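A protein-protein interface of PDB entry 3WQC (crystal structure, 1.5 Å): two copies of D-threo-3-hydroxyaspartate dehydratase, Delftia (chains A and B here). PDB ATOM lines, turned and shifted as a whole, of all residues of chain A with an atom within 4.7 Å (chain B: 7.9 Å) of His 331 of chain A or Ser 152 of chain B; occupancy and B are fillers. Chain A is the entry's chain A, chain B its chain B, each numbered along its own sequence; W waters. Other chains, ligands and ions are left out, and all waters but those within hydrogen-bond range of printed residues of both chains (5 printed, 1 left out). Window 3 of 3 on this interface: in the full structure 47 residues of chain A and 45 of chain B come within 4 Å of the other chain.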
ATOM      1  N   ILE A 275      34.066  21.214   0.463  1.00  0.00           N
ATOM      2  CA  ILE A 275      34.174  20.723   1.866  1.00  0.00           C
ATOM      3  C   ILE A 275      34.456  19.220   1.916  1.00  0.00           C
ATOM      4  O   ILE A 275      34.690  18.680   2.988  1.00  0.00           O
ATOM      5  CB  ILE A 275      32.875  20.995   2.627  1.00  0.00           C
ATOM      6  CG1 ILE A 275      31.648  20.321   1.990  1.00  0.00           C
ATOM      7  CG2 ILE A 275      32.713  22.534   2.761  1.00  0.00           C
ATOM      8  CD1 ILE A 275      30.348  20.533   2.854  1.00  0.00           C
ATOM      9  N   GLN A 278      33.992  12.481  -2.905  1.00  0.00           N
ATOM     10  CA  GLN A 278      33.850  10.977  -2.955  1.00  0.00           C
ATOM     11  C   GLN A 278      34.653  10.610  -4.170  1.00  0.00           C
ATOM     12  O   GLN A 278      34.173  10.686  -5.314  1.00  0.00           O
ATOM     13  CB  GLN A 278      32.422  10.459  -3.085  1.00  0.00           C
ATOM     14  CG  GLN A 278      31.641  10.518  -1.808  1.00  0.00           C
ATOM     15  CD  GLN A 278      32.232   9.781  -0.607  1.00  0.00           C
ATOM     16  OE1 GLN A 278      33.168   8.986  -0.712  1.00  0.00           O
ATOM     17  NE2 GLN A 278      31.668  10.006   0.544  1.00  0.00           N
ATOM     18  N   ILE A 285      32.257  17.663  -3.002  1.00  0.00           N
ATOM     19  CA  ILE A 285      31.060  18.097  -2.232  1.00  0.00           C
ATOM     20  C   ILE A 285      31.310  19.562  -1.858  1.00  0.00           C
ATOM     21  O   ILE A 285      32.397  19.940  -1.356  1.00  0.00           O
ATOM     22  CB  ILE A 285      30.905  17.309  -0.976  1.00  0.00           C
ATOM     23  CG1 ILE A 285      31.012  15.858  -1.276  1.00  0.00           C
ATOM     24  CG2 ILE A 285      29.639  17.750  -0.210  1.00  0.00           C
ATOM     25  CD1 ILE A 285      29.962  15.418  -2.049  1.00  0.00           C
ATOM     26  N   VAL A 286      30.314  20.437  -2.182  1.00  0.00           N
ATOM     27  CA  VAL A 286      30.436  21.864  -1.885  1.00  0.00           C
ATOM     28  C   VAL A 286      29.367  22.218  -0.864  1.00  0.00           C
ATOM     29  O   VAL A 286      28.389  21.490  -0.649  1.00  0.00           O
ATOM     30  CB  VAL A 286      30.301  22.749  -3.154  1.00  0.00           C
ATOM     31  CG1 VAL A 286      31.500  22.494  -4.068  1.00  0.00           C
ATOM     32  CG2 VAL A 286      28.963  22.516  -3.906  1.00  0.00           C
ATOM     33  N   ALA A 288      27.214  24.583  -1.097  1.00  0.00           N
ATOM     34  CA  ALA A 288      26.014  25.153  -1.758  1.00  0.00           C
ATOM     35  C   ALA A 288      25.100  23.994  -2.113  1.00  0.00           C
ATOM     36  O   ALA A 288      25.314  23.324  -3.145  1.00  0.00           O
ATOM     37  CB  ALA A 288      26.417  25.974  -2.982  1.00  0.00           C
ATOM     38  N   GLY A 289      24.138  23.700  -1.214  1.00  0.00           N
ATOM     39  CA  GLY A 289      23.118  22.727  -1.556  1.00  0.00           C
ATOM     40  C   GLY A 289      21.858  23.413  -2.100  1.00  0.00           C
ATOM     41  O   GLY A 289      21.943  24.569  -2.576  1.00  0.00           O
ATOM     42  N   GLY A 326      23.799  16.930  -8.157  1.00  0.00           N
ATOM     43  CA  GLY A 326      22.803  16.616  -7.111  1.00  0.00           C
ATOM     44  C   GLY A 326      22.918  17.672  -6.002  1.00  0.00           C
ATOM     45  O   GLY A 326      23.903  18.414  -5.949  1.00  0.00           O
ATOM     46  N   ALA A 327      21.930  17.685  -5.118  1.00  0.00           N
ATOM     47  CA  ALA A 327      21.966  18.640  -3.975  1.00  0.00           C
ATOM     48  C   ALA A 327      21.092  18.127  -2.870  1.00  0.00           C
ATOM     49  O   ALA A 327      19.952  17.644  -3.114  1.00  0.00           O
ATOM     50  CB  ALA A 327      21.481  20.015  -4.420  1.00  0.00           C
ATOM     51  N   ASN A 328      21.600  18.216  -1.643  1.00  0.00           N
ATOM     52  CA  ASN A 328      20.782  18.102  -0.445  1.00  0.00           C
ATOM     53  C   ASN A 328      20.730  19.473   0.202  1.00  0.00           C
ATOM     54  O   ASN A 328      21.174  20.451  -0.430  1.00  0.00           O
ATOM     55  CB  ASN A 328      21.306  17.035   0.457  1.00  0.00           C
ATOM     56  CG  ASN A 328      21.142  15.605  -0.111  1.00  0.00           C
ATOM     57  OD1 ASN A 328      21.644  14.746   0.429  1.00  0.00           O
ATOM     58  ND2 ASN A 328      20.258  15.366  -1.096  1.00  0.00           N
ATOM     59  N   GLN A 329      20.248  19.622   1.408  1.00  0.00           N
ATOM     60  CA  GLN A 329      19.920  20.978   1.885  1.00  0.00           C
ATOM     61  C   GLN A 329      21.152  21.897   1.916  1.00  0.00           C
ATOM     62  O   GLN A 329      21.124  23.022   1.405  1.00  0.00           O
ATOM     63  CB  GLN A 329      19.232  20.844   3.267  1.00  0.00           C
ATOM     64  CG  GLN A 329      18.683  22.187   3.758  1.00  0.00           C
ATOM     65  CD  GLN A 329      17.710  21.955   4.944  1.00  0.00           C
ATOM     66  OE1 GLN A 329      16.909  20.966   4.923  1.00  0.00           O
ATOM     67  NE2 GLN A 329      17.664  22.912   5.903  1.00  0.00           N
ATOM     68  N   GLU A 330      22.261  21.381   2.559  1.00  0.00           N
ATOM     69  CA  GLU A 330      23.483  22.194   2.733  1.00  0.00           C
ATOM     70  C   GLU A 330      24.685  21.547   2.062  1.00  0.00           C
ATOM     71  O   GLU A 330      25.819  21.998   2.314  1.00  0.00           O
ATOM     72  CB  GLU A 330      23.763  22.453   4.220  1.00  0.00           C
ATOM     73  CG  GLU A 330      22.694  23.435   4.861  1.00  0.00           C
ATOM     74  CD  GLU A 330      22.719  24.856   4.285  1.00  0.00           C
ATOM     75  OE1 GLU A 330      23.726  25.316   3.674  1.00  0.00           O
ATOM     76  OE2 GLU A 330      21.673  25.569   4.485  1.00  0.00           O
ATOM     77  N   HIS A 331      24.440  20.568   1.165  1.00  0.00           N
ATOM     78  CA  HIS A 331      25.545  19.936   0.428  1.00  0.00           C
ATOM     79  C   HIS A 331      25.213  19.884  -1.016  1.00  0.00           C
ATOM     80  O   HIS A 331      24.107  19.453  -1.410  1.00  0.00           O
ATOM     81  CB  HIS A 331      25.640  18.386   0.797  1.00  0.00           C
ATOM     82  CG  HIS A 331      25.954  18.092   2.207  1.00  0.00           C
ATOM     83  ND1 HIS A 331      25.041  18.204   3.246  1.00  0.00           N
ATOM     84  CD2 HIS A 331      27.160  17.666   2.806  1.00  0.00           C
ATOM     85  CE1 HIS A 331      25.608  17.803   4.428  1.00  0.00           C
ATOM     86  NE2 HIS A 331      26.851  17.404   4.166  1.00  0.00           N
ATOM     87  N   GLY A 332      26.093  20.360  -1.878  1.00  0.00           N
ATOM     88  CA  GLY A 332      25.929  20.207  -3.313  1.00  0.00           C
ATOM     89  C   GLY A 332      26.958  19.151  -3.781  1.00  0.00           C
ATOM     90  O   GLY A 332      28.080  19.069  -3.306  1.00  0.00           O
ATOM     91  N   ILE A 333      26.571  18.406  -4.842  1.00  0.00           N
ATOM     92  CA  ILE A 333      27.454  17.378  -5.397  1.00  0.00           C
ATOM     93  C   ILE A 333      27.936  17.893  -6.724  1.00  0.00           C
ATOM     94  O   ILE A 333      27.102  18.001  -7.685  1.00  0.00           O
ATOM     95  CB  ILE A 333      26.736  16.038  -5.575  1.00  0.00           C
ATOM     96  CG1 ILE A 333      26.139  15.556  -4.274  1.00  0.00           C
ATOM     97  CG2 ILE A 333      27.719  15.019  -6.248  1.00  0.00           C
ATOM     98  CD1 ILE A 333      27.008  15.378  -3.238  1.00  0.00           C
ATOM     99  N   HIS B  51      17.340  17.171  14.620  1.00  0.00           N
ATOM    100  CA  HIS B  51      17.979  18.075  13.615  1.00  0.00           C
ATOM    101  C   HIS B  51      17.085  19.266  13.383  1.00  0.00           C
ATOM    102  O   HIS B  51      15.980  19.112  12.854  1.00  0.00           O
ATOM    103  CB  HIS B  51      18.234  17.288  12.296  1.00  0.00           C
ATOM    104  CG  HIS B  51      19.371  17.916  11.562  1.00  0.00           C
ATOM    105  ND1 HIS B  51      19.448  19.303  11.365  1.00  0.00           N
ATOM    106  CD2 HIS B  51      20.543  17.360  11.003  1.00  0.00           C
ATOM    107  CE1 HIS B  51      20.624  19.592  10.784  1.00  0.00           C
ATOM    108  NE2 HIS B  51      21.265  18.398  10.512  1.00  0.00           N
ATOM    109  N   LYS B  53      17.412  21.641  11.336  1.00  0.00           N
ATOM    110  CA  LYS B  53      17.442  22.286  10.027  1.00  0.00           C
ATOM    111  C   LYS B  53      16.043  22.321   9.411  1.00  0.00           C
ATOM    112  O   LYS B  53      15.787  23.144   8.496  1.00  0.00           O
ATOM    113  CB  LYS B  53      18.381  21.608   9.071  1.00  0.00           C
ATOM    114  CG  LYS B  53      17.902  20.263   8.542  1.00  0.00           C
ATOM    115  CD  LYS B  53      19.038  19.733   7.645  1.00  0.00           C
ATOM    116  CE  LYS B  53      18.505  18.507   6.969  1.00  0.00           C
ATOM    117  NZ  LYS B  53      19.412  17.339   7.070  1.00  0.00           N
ATOM    118  N   SER B  75      22.631  22.418  10.709  1.00  0.00           N
ATOM    119  CA  SER B  75      23.160  22.319   9.330  1.00  0.00           C
ATOM    120  C   SER B  75      24.059  23.502   8.968  1.00  0.00           C
ATOM    121  O   SER B  75      24.615  23.481   7.857  1.00  0.00           O
ATOM    122  CB  SER B  75      22.050  22.167   8.306  1.00  0.00           C
ATOM    123  OG  SER B  75      21.303  23.387   8.147  1.00  0.00           O
ATOM    124  N   TYR B  93      27.393  20.180  14.658  1.00  0.00           N
ATOM    125  CA  TYR B  93      27.319  20.793  13.338  1.00  0.00           C
ATOM    126  C   TYR B  93      27.628  19.714  12.314  1.00  0.00           C
ATOM    127  O   TYR B  93      28.793  19.314  12.104  1.00  0.00           O
ATOM    128  CB  TYR B  93      28.305  21.960  13.259  1.00  0.00           C
ATOM    129  CG  TYR B  93      28.432  22.517  11.861  1.00  0.00           C
ATOM    130  CD1 TYR B  93      27.353  22.653  10.956  1.00  0.00           C
ATOM    131  CD2 TYR B  93      29.723  22.914  11.437  1.00  0.00           C
ATOM    132  CE1 TYR B  93      27.562  23.186   9.643  1.00  0.00           C
ATOM    133  CE2 TYR B  93      29.927  23.479  10.169  1.00  0.00           C
ATOM    134  CZ  TYR B  93      28.854  23.602   9.286  1.00  0.00           C
ATOM    135  OH  TYR B  93      29.044  24.101   8.016  1.00  0.00           O
ATOM    136  N   ALA B  94      26.557  19.121  11.726  1.00  0.00           N
ATOM    137  CA  ALA B  94      26.691  17.847  10.966  1.00  0.00           C
ATOM    138  C   ALA B  94      26.852  18.130   9.467  1.00  0.00           C
ATOM    139  O   ALA B  94      26.129  17.540   8.627  1.00  0.00           O
ATOM    140  CB  ALA B  94      25.507  16.901  11.264  1.00  0.00           C
ATOM    141  N   VAL B  95      27.827  18.969   9.130  1.00  0.00           N
ATOM    142  CA  VAL B  95      28.217  19.162   7.713  1.00  0.00           C
ATOM    143  C   VAL B  95      29.767  19.162   7.756  1.00  0.00           C
ATOM    144  O   VAL B  95      30.331  19.850   8.590  1.00  0.00           O
ATOM    145  CB  VAL B  95      27.724  20.530   7.130  1.00  0.00           C
ATOM    146  CG1 VAL B  95      28.231  20.748   5.712  1.00  0.00           C
ATOM    147  CG2 VAL B  95      26.175  20.532   7.142  1.00  0.00           C
ATOM    148  N   SER B  96      30.401  18.423   6.831  1.00  0.00           N
ATOM    149  CA  SER B  96      31.878  18.306   6.776  1.00  0.00           C
ATOM    150  C   SER B  96      32.487  19.692   6.989  1.00  0.00           C
ATOM    151  O   SER B  96      32.183  20.656   6.262  1.00  0.00           O
ATOM    152  CB  SER B  96      32.266  17.845   5.356  1.00  0.00           C
ATOM    153  OG  SER B  96      31.685  16.636   4.986  1.00  0.00           O
ATOM    154  N   ILE B 118      32.434  17.768  12.370  1.00  0.00           N
ATOM    155  CA  ILE B 118      32.580  16.461  11.738  1.00  0.00           C
ATOM    156  C   ILE B 118      33.546  16.598  10.582  1.00  0.00           C
ATOM    157  O   ILE B 118      33.643  17.646   9.915  1.00  0.00           O
ATOM    158  CB  ILE B 118      31.215  15.857  11.293  1.00  0.00           C
ATOM    159  CG1 ILE B 118      30.648  16.525  10.041  1.00  0.00           C
ATOM    160  CG2 ILE B 118      30.217  15.876  12.478  1.00  0.00           C
ATOM    161  CD1 ILE B 118      29.401  15.780   9.512  1.00  0.00           C
ATOM    162  N   VAL B 119      34.262  15.502  10.289  1.00  0.00           N
ATOM    163  CA  VAL B 119      35.164  15.438   9.121  1.00  0.00           C
ATOM    164  C   VAL B 119      35.035  14.052   8.489  1.00  0.00           C
ATOM    165  O   VAL B 119      34.636  13.075   9.149  1.00  0.00           O
ATOM    166  CB  VAL B 119      36.672  15.719   9.441  1.00  0.00           C
ATOM    167  CG1 VAL B 119      36.812  17.117  10.038  1.00  0.00           C
ATOM    168  CG2 VAL B 119      37.271  14.666  10.355  1.00  0.00           C
ATOM    169  N   ASP B 120      35.577  13.936   7.276  1.00  0.00           N
ATOM    170  CA  ASP B 120      35.685  12.635   6.574  1.00  0.00           C
ATOM    171  C   ASP B 120      36.965  12.514   5.758  1.00  0.00           C
ATOM    172  O   ASP B 120      37.032  11.632   4.868  1.00  0.00           O
ATOM    173  CB  ASP B 120      34.456  12.317   5.729  1.00  0.00           C
ATOM    174  CG  ASP B 120      34.307  13.195   4.541  1.00  0.00           C
ATOM    175  OD1 ASP B 120      35.122  14.111   4.301  1.00  0.00           O
ATOM    176  OD2 ASP B 120      33.333  12.967   3.747  1.00  0.00           O
ATOM    177  N   GLU B 144      32.577  11.284  10.037  1.00  0.00           N
ATOM    178  CA  GLU B 144      31.369  10.900   9.280  1.00  0.00           C
ATOM    179  C   GLU B 144      31.579   9.612   8.460  1.00  0.00           C
ATOM    180  O   GLU B 144      32.634   9.498   7.795  1.00  0.00           O
ATOM    181  CB  GLU B 144      30.926  12.062   8.355  1.00  0.00           C
ATOM    182  CG  GLU B 144      29.544  11.776   7.687  1.00  0.00           C
ATOM    183  CD  GLU B 144      28.917  12.949   6.997  1.00  0.00           C
ATOM    184  OE1 GLU B 144      27.685  12.819   6.742  1.00  0.00           O
ATOM    185  OE2 GLU B 144      29.638  13.931   6.677  1.00  0.00           O
ATOM    186  N   ILE B 145      30.617   8.681   8.519  1.00  0.00           N
ATOM    187  CA  ILE B 145      30.724   7.363   7.914  1.00  0.00           C
ATOM    188  C   ILE B 145      29.690   7.328   6.775  1.00  0.00           C
ATOM    189  O   ILE B 145      28.533   7.745   6.942  1.00  0.00           O
ATOM    190  CB  ILE B 145      30.421   6.278   8.954  1.00  0.00           C
ATOM    191  CG1 ILE B 145      31.340   6.444  10.185  1.00  0.00           C
ATOM    192  CG2 ILE B 145      30.584   4.882   8.288  1.00  0.00           C
ATOM    193  CD1 ILE B 145      32.839   6.454   9.882  1.00  0.00           C
ATOM    194  N   ASP B 146      30.085   6.790   5.636  1.00  0.00           N
ATOM    195  CA  ASP B 146      29.186   6.569   4.484  1.00  0.00           C
ATOM    196  C   ASP B 146      28.720   5.111   4.618  1.00  0.00           C
ATOM    197  O   ASP B 146      29.529   4.153   4.491  1.00  0.00           O
ATOM    198  CB  ASP B 146      29.978   6.724   3.181  1.00  0.00           C
ATOM    199  CG  ASP B 146      29.152   6.425   1.958  1.00  0.00           C
ATOM    200  OD1 ASP B 146      27.957   6.110   2.130  1.00  0.00           O
ATOM    201  OD2 ASP B 146      29.713   6.470   0.827  1.00  0.00           O
ATOM    202  N   THR B 147      27.460   4.898   5.002  1.00  0.00           N
ATOM    203  CA  THR B 147      26.913   3.555   5.183  1.00  0.00           C
ATOM    204  C   THR B 147      26.008   3.157   4.032  1.00  0.00           C
ATOM    205  O   THR B 147      25.679   1.966   3.920  1.00  0.00           O
ATOM    206  CB  THR B 147      26.136   3.408   6.519  1.00  0.00           C
ATOM    207  OG1 THR B 147      25.093   4.425   6.594  1.00  0.00           O
ATOM    208  CG2 THR B 147      27.062   3.551   7.708  1.00  0.00           C
ATOM    209  N   ASP B 148      25.604   4.094   3.149  1.00  0.00           N
ATOM    210  CA  ASP B 148      24.680   3.752   2.059  1.00  0.00           C
ATOM    211  C   ASP B 148      24.931   4.394   0.680  1.00  0.00           C
ATOM    212  O   ASP B 148      24.075   4.265  -0.229  1.00  0.00           O
ATOM    213  CB  ASP B 148      23.243   4.026   2.537  1.00  0.00           C
ATOM    214  CG  ASP B 148      22.984   5.550   2.601  1.00  0.00           C
ATOM    215  OD1 ASP B 148      24.001   6.325   2.631  1.00  0.00           O
ATOM    216  OD2 ASP B 148      21.781   5.946   2.657  1.00  0.00           O
ATOM    217  N   GLY B 149      26.079   5.093   0.499  1.00  0.00           N
ATOM    218  CA  GLY B 149      26.439   5.716  -0.740  1.00  0.00           C
ATOM    219  C   GLY B 149      25.753   7.035  -1.022  1.00  0.00           C
ATOM    220  O   GLY B 149      25.805   7.538  -2.130  1.00  0.00           O
ATOM    221  N   HIS B 150      25.051   7.570  -0.020  1.00  0.00           N
ATOM    222  CA  HIS B 150      24.224   8.740  -0.223  1.00  0.00           C
ATOM    223  C   HIS B 150      25.025  10.007  -0.511  1.00  0.00           C
ATOM    224  O   HIS B 150      24.620  10.779  -1.460  1.00  0.00           O
ATOM    225  CB  HIS B 150      23.332   8.966   1.053  1.00  0.00           C
ATOM    226  CG  HIS B 150      22.450  10.149   0.971  1.00  0.00           C
ATOM    227  ND1 HIS B 150      21.402  10.244   0.047  1.00  0.00           N
ATOM    228  CD2 HIS B 150      22.365  11.292   1.814  1.00  0.00           C
ATOM    229  CE1 HIS B 150      20.763  11.465   0.258  1.00  0.00           C
ATOM    230  NE2 HIS B 150      21.333  12.079   1.329  1.00  0.00           N
ATOM    231  N   ARG B 151      26.063  10.310   0.298  1.00  0.00           N
ATOM    232  CA  ARG B 151      26.596  11.685   0.280  1.00  0.00           C
ATOM    233  C   ARG B 151      28.040  11.623   0.916  1.00  0.00           C
ATOM    234  O   ARG B 151      28.873  11.032   0.316  1.00  0.00           O
ATOM    235  CB  ARG B 151      25.686  12.630   1.138  1.00  0.00           C
ATOM    236  CG  ARG B 151      25.937  14.141   0.935  1.00  0.00           C
ATOM    237  CD  ARG B 151      24.756  14.815   1.621  1.00  0.00           C
ATOM    238  NE  ARG B 151      24.737  14.685   3.069  1.00  0.00           N
ATOM    239  CZ  ARG B 151      23.652  14.990   3.859  1.00  0.00           C
ATOM    240  NH1 ARG B 151      22.464  15.296   3.286  1.00  0.00           N
ATOM    241  NH2 ARG B 151      23.780  15.024   5.196  1.00  0.00           N
ATOM    242  N   SER B 152      28.367  12.310   2.019  1.00  0.00           N
ATOM    243  CA  SER B 152      29.732  12.397   2.559  1.00  0.00           C
ATOM    244  C   SER B 152      30.048  11.187   3.429  1.00  0.00           C
ATOM    245  O   SER B 152      29.192  10.259   3.684  1.00  0.00           O
ATOM    246  CB  SER B 152      29.820  13.630   3.480  1.00  0.00           C
ATOM    247  OG  SER B 152      29.548  14.826   2.732  1.00  0.00           O
ATOM    248  N   GLY B 153      31.329  11.054   3.806  1.00  0.00           N
ATOM    249  CA  GLY B 153      31.648  10.011   4.766  1.00  0.00           C
ATOM    250  C   GLY B 153      32.718   9.033   4.277  1.00  0.00           C
ATOM    251  O   GLY B 153      32.876   8.702   3.094  1.00  0.00           O
ATOM    252  N   VAL B 154      33.468   8.555   5.265  1.00  0.00           N
ATOM    253  CA  VAL B 154      34.451   7.479   5.044  1.00  0.00           C
ATOM    254  C   VAL B 154      33.668   6.186   4.881  1.00  0.00           C
ATOM    255  O   VAL B 154      32.735   5.904   5.720  1.00  0.00           O
ATOM    256  CB  VAL B 154      35.354   7.392   6.325  1.00  0.00           C
ATOM    257  CG1 VAL B 154      36.384   6.263   6.147  1.00  0.00           C
ATOM    258  CG2 VAL B 154      35.994   8.741   6.599  1.00  0.00           C
ATOM    259  N   GLY B 155      34.053   5.313   3.963  1.00  0.00           N
ATOM    260  CA  GLY B 155      33.358   4.006   3.950  1.00  0.00           C
ATOM    261  C   GLY B 155      33.492   3.236   5.250  1.00  0.00           C
ATOM    262  O   GLY B 155      34.578   3.231   5.901  1.00  0.00           O
ATOM    263  N   LEU B 180      29.420   9.283  13.074  1.00  0.00           N
ATOM    264  CA  LEU B 180      28.022   9.482  12.770  1.00  0.00           C
ATOM    265  C   LEU B 180      27.779   9.063  11.318  1.00  0.00           C
ATOM    266  O   LEU B 180      28.717   9.143  10.475  1.00  0.00           O
ATOM    267  CB  LEU B 180      27.542  10.951  12.971  1.00  0.00           C
ATOM    268  CG  LEU B 180      28.003  11.983  11.924  1.00  0.00           C
ATOM    269  CD1 LEU B 180      27.106  13.252  12.028  1.00  0.00           C
ATOM    270  CD2 LEU B 180      29.493  12.398  12.070  1.00  0.00           C
ATOM    271  N   THR B 181      26.519   8.732  10.994  1.00  0.00           N
ATOM    272  CA  THR B 181      26.171   8.425   9.629  1.00  0.00           C
ATOM    273  C   THR B 181      24.739   8.924   9.415  1.00  0.00           C
ATOM    274  O   THR B 181      23.965   8.995  10.416  1.00  0.00           O
ATOM    275  CB  THR B 181      26.262   6.894   9.298  1.00  0.00           C
ATOM    276  OG1 THR B 181      26.149   6.784   7.861  1.00  0.00           O
ATOM    277  CG2 THR B 181      25.192   6.107   9.978  1.00  0.00           C
ATOM    278  N   HIS B 182      24.395   9.245   8.155  1.00  0.00           N
ATOM    279  CA  HIS B 182      23.034   9.584   7.800  1.00  0.00           C
ATOM    280  C   HIS B 182      22.650   8.795   6.628  1.00  0.00           C
ATOM    281  O   HIS B 182      23.220   8.998   5.485  1.00  0.00           O
ATOM    282  CB  HIS B 182      23.040  11.089   7.442  1.00  0.00           C
ATOM    283  CG  HIS B 182      21.767  11.609   6.829  1.00  0.00           C
ATOM    284  ND1 HIS B 182      20.500  11.589   7.457  1.00  0.00           N
ATOM    285  CD2 HIS B 182      21.565  12.205   5.561  1.00  0.00           C
ATOM    286  CE1 HIS B 182      19.599  12.224   6.588  1.00  0.00           C
ATOM    287  NE2 HIS B 182      20.215  12.538   5.475  1.00  0.00           N
HETATM  288  O   HOH W   1      19.913  24.664   6.116  1.00  0.00           O
HETATM  289  O   HOH W   2      29.036  16.246   5.427  1.00  0.00           O
HETATM  290  O   HOH W   3      23.208  13.340  -1.815  1.00  0.00           O
HETATM  291  O   HOH W   4      35.599   8.390   1.328  1.00  0.00           O
HETATM  292  O   HOH W   5      26.271  15.346   6.725  1.00  0.00           O
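The side-chain amide nitrogen (NE2) of Gln 278 of chain A is in hydrogen-bond range of the backbone carbonyl oxygen (O) of Arg 151 of chain B (3.0 Å). O of Gly 153 of chain B is in hydrogen-bond range of NE2 of Gln 278 of chain A (3.1 Å). OD1 of Asn 328 of chain A sits at hydrogen-bond distance from NE2 of His 150 of chain B (2.8 Å). The side-chain amide oxygen (OD1) of Asn 328 of chain A lies within hydrogen-bond range of the guanidinium group (NH1) of Arg 151 of chain B, at 3.0 Å. NE2 of Gln 329 of chain A lies within hydrogen-bond range of O of Lys 53 of chain B (3.2 Å).
The backbone NH (N) of Ile 275 of chain A sits at hydrogen-bond distance from the backbone carbonyl oxygen (O) of Ile 285 of chain A, at 2.8 Å. ND1 of His 51 of chain B lies within hydrogen-bond range of N of Lys 53 of chain B (3.1 Å). OD2 of Asp 120 of chain B lies within hydrogen-bond range of N of Gly 153 of chain B. OD1 of Asp 148 of chain B is in hydrogen-bond range of N of His 150 of chain B (3.1 Å).
Among the printed residues, pairs that only touch across the chains: Ile 275 of chain A with Val 95 of chain B, Ile 275 of chain A with Ser 96 of chain B, Gln 278 of chain A with Ser 152 of chain B, Glu 330 of chain A with Ser 75 of chain B, His 331 of chain A with Val 95 of chain B, His 331 of chain A with Arg 151 of chain B and His 331 of chain A with Ser 152 of chain B.
His 331 of chain A touches just these residues of chain B: Val 95, Arg 151 and Ser 152. Ser 152 of chain B touches two residues of chain A. No residue of chain B comes within 4 Å of Gly 332 of chain A. Of the printed residues of chain A, His 150 of chain B touches Asn 328 (2.8 Å). Of the printed residues of chain A, Ser 96 of chain B touches Ile 275. Printed residues of chain A within 4 Å of Lys 53 of chain B: Gln 329 (3.2 Å). Ile 118 of chain B touches none of the printed residues of chain A. The nearest residue of chain B that does not touch His 331 of chain A is Ala 94 of chain B (4.2 Å). The nearest residue of chain A that does not touch Ser 152 of chain B is Ile 285 of chain A (4.1 Å).
Of the 25 printed residues of chain B, 8 touch a printed residue of chain A. Of the 14 printed residues of chain A, 6 touch a printed residue of chain B. Hydrophobic or aromatic side chains of chain A that line the printed part of chain B: Ile 275 and His 331. Among the printed residues, 12 pairs touch across the chains. Among the printed residues, no Asp or Glu carboxylate lies within 4 Å of a Lys or Arg side-chain nitrogen of the other chain.
No position is printed for both chains. Of the 12 pairs that touch across the chains among the printed residues, none has its exchanged pair printed and touching as well.
Water W1 lies within hydrogen-bond range of OE2 of Glu 330 of chain A, OG of Ser 75 of chain B and NE2 of Gln 329 of chain A. Water W2 lies within hydrogen-bond range of OE2 of Glu 144 of chain B, OG of Ser 96 of chain B, NE2 of His 331 of chain A and OG of Ser 152 of chain B. Water W5 lies within hydrogen-bond range of the side-chain carboxylate (OE1) of Glu 144 of chain B, the backbone carbonyl oxygen (O) of Ala 94 of chain B, the guanidinium group (NH2) of Arg 151 of chain B and a ring nitrogen (NE2) of His 331 of chain A. Water W3 lies within hydrogen-bond range of O of His 150 of chain B (2.9 Å) and OD1 of Asn 328 of chain A (3.1 Å). Water W4 lies within hydrogen-bond range of OE1 of Gln 278 of chain A (3.2 Å) and O of Gly 153 of chain B (3.3 Å).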
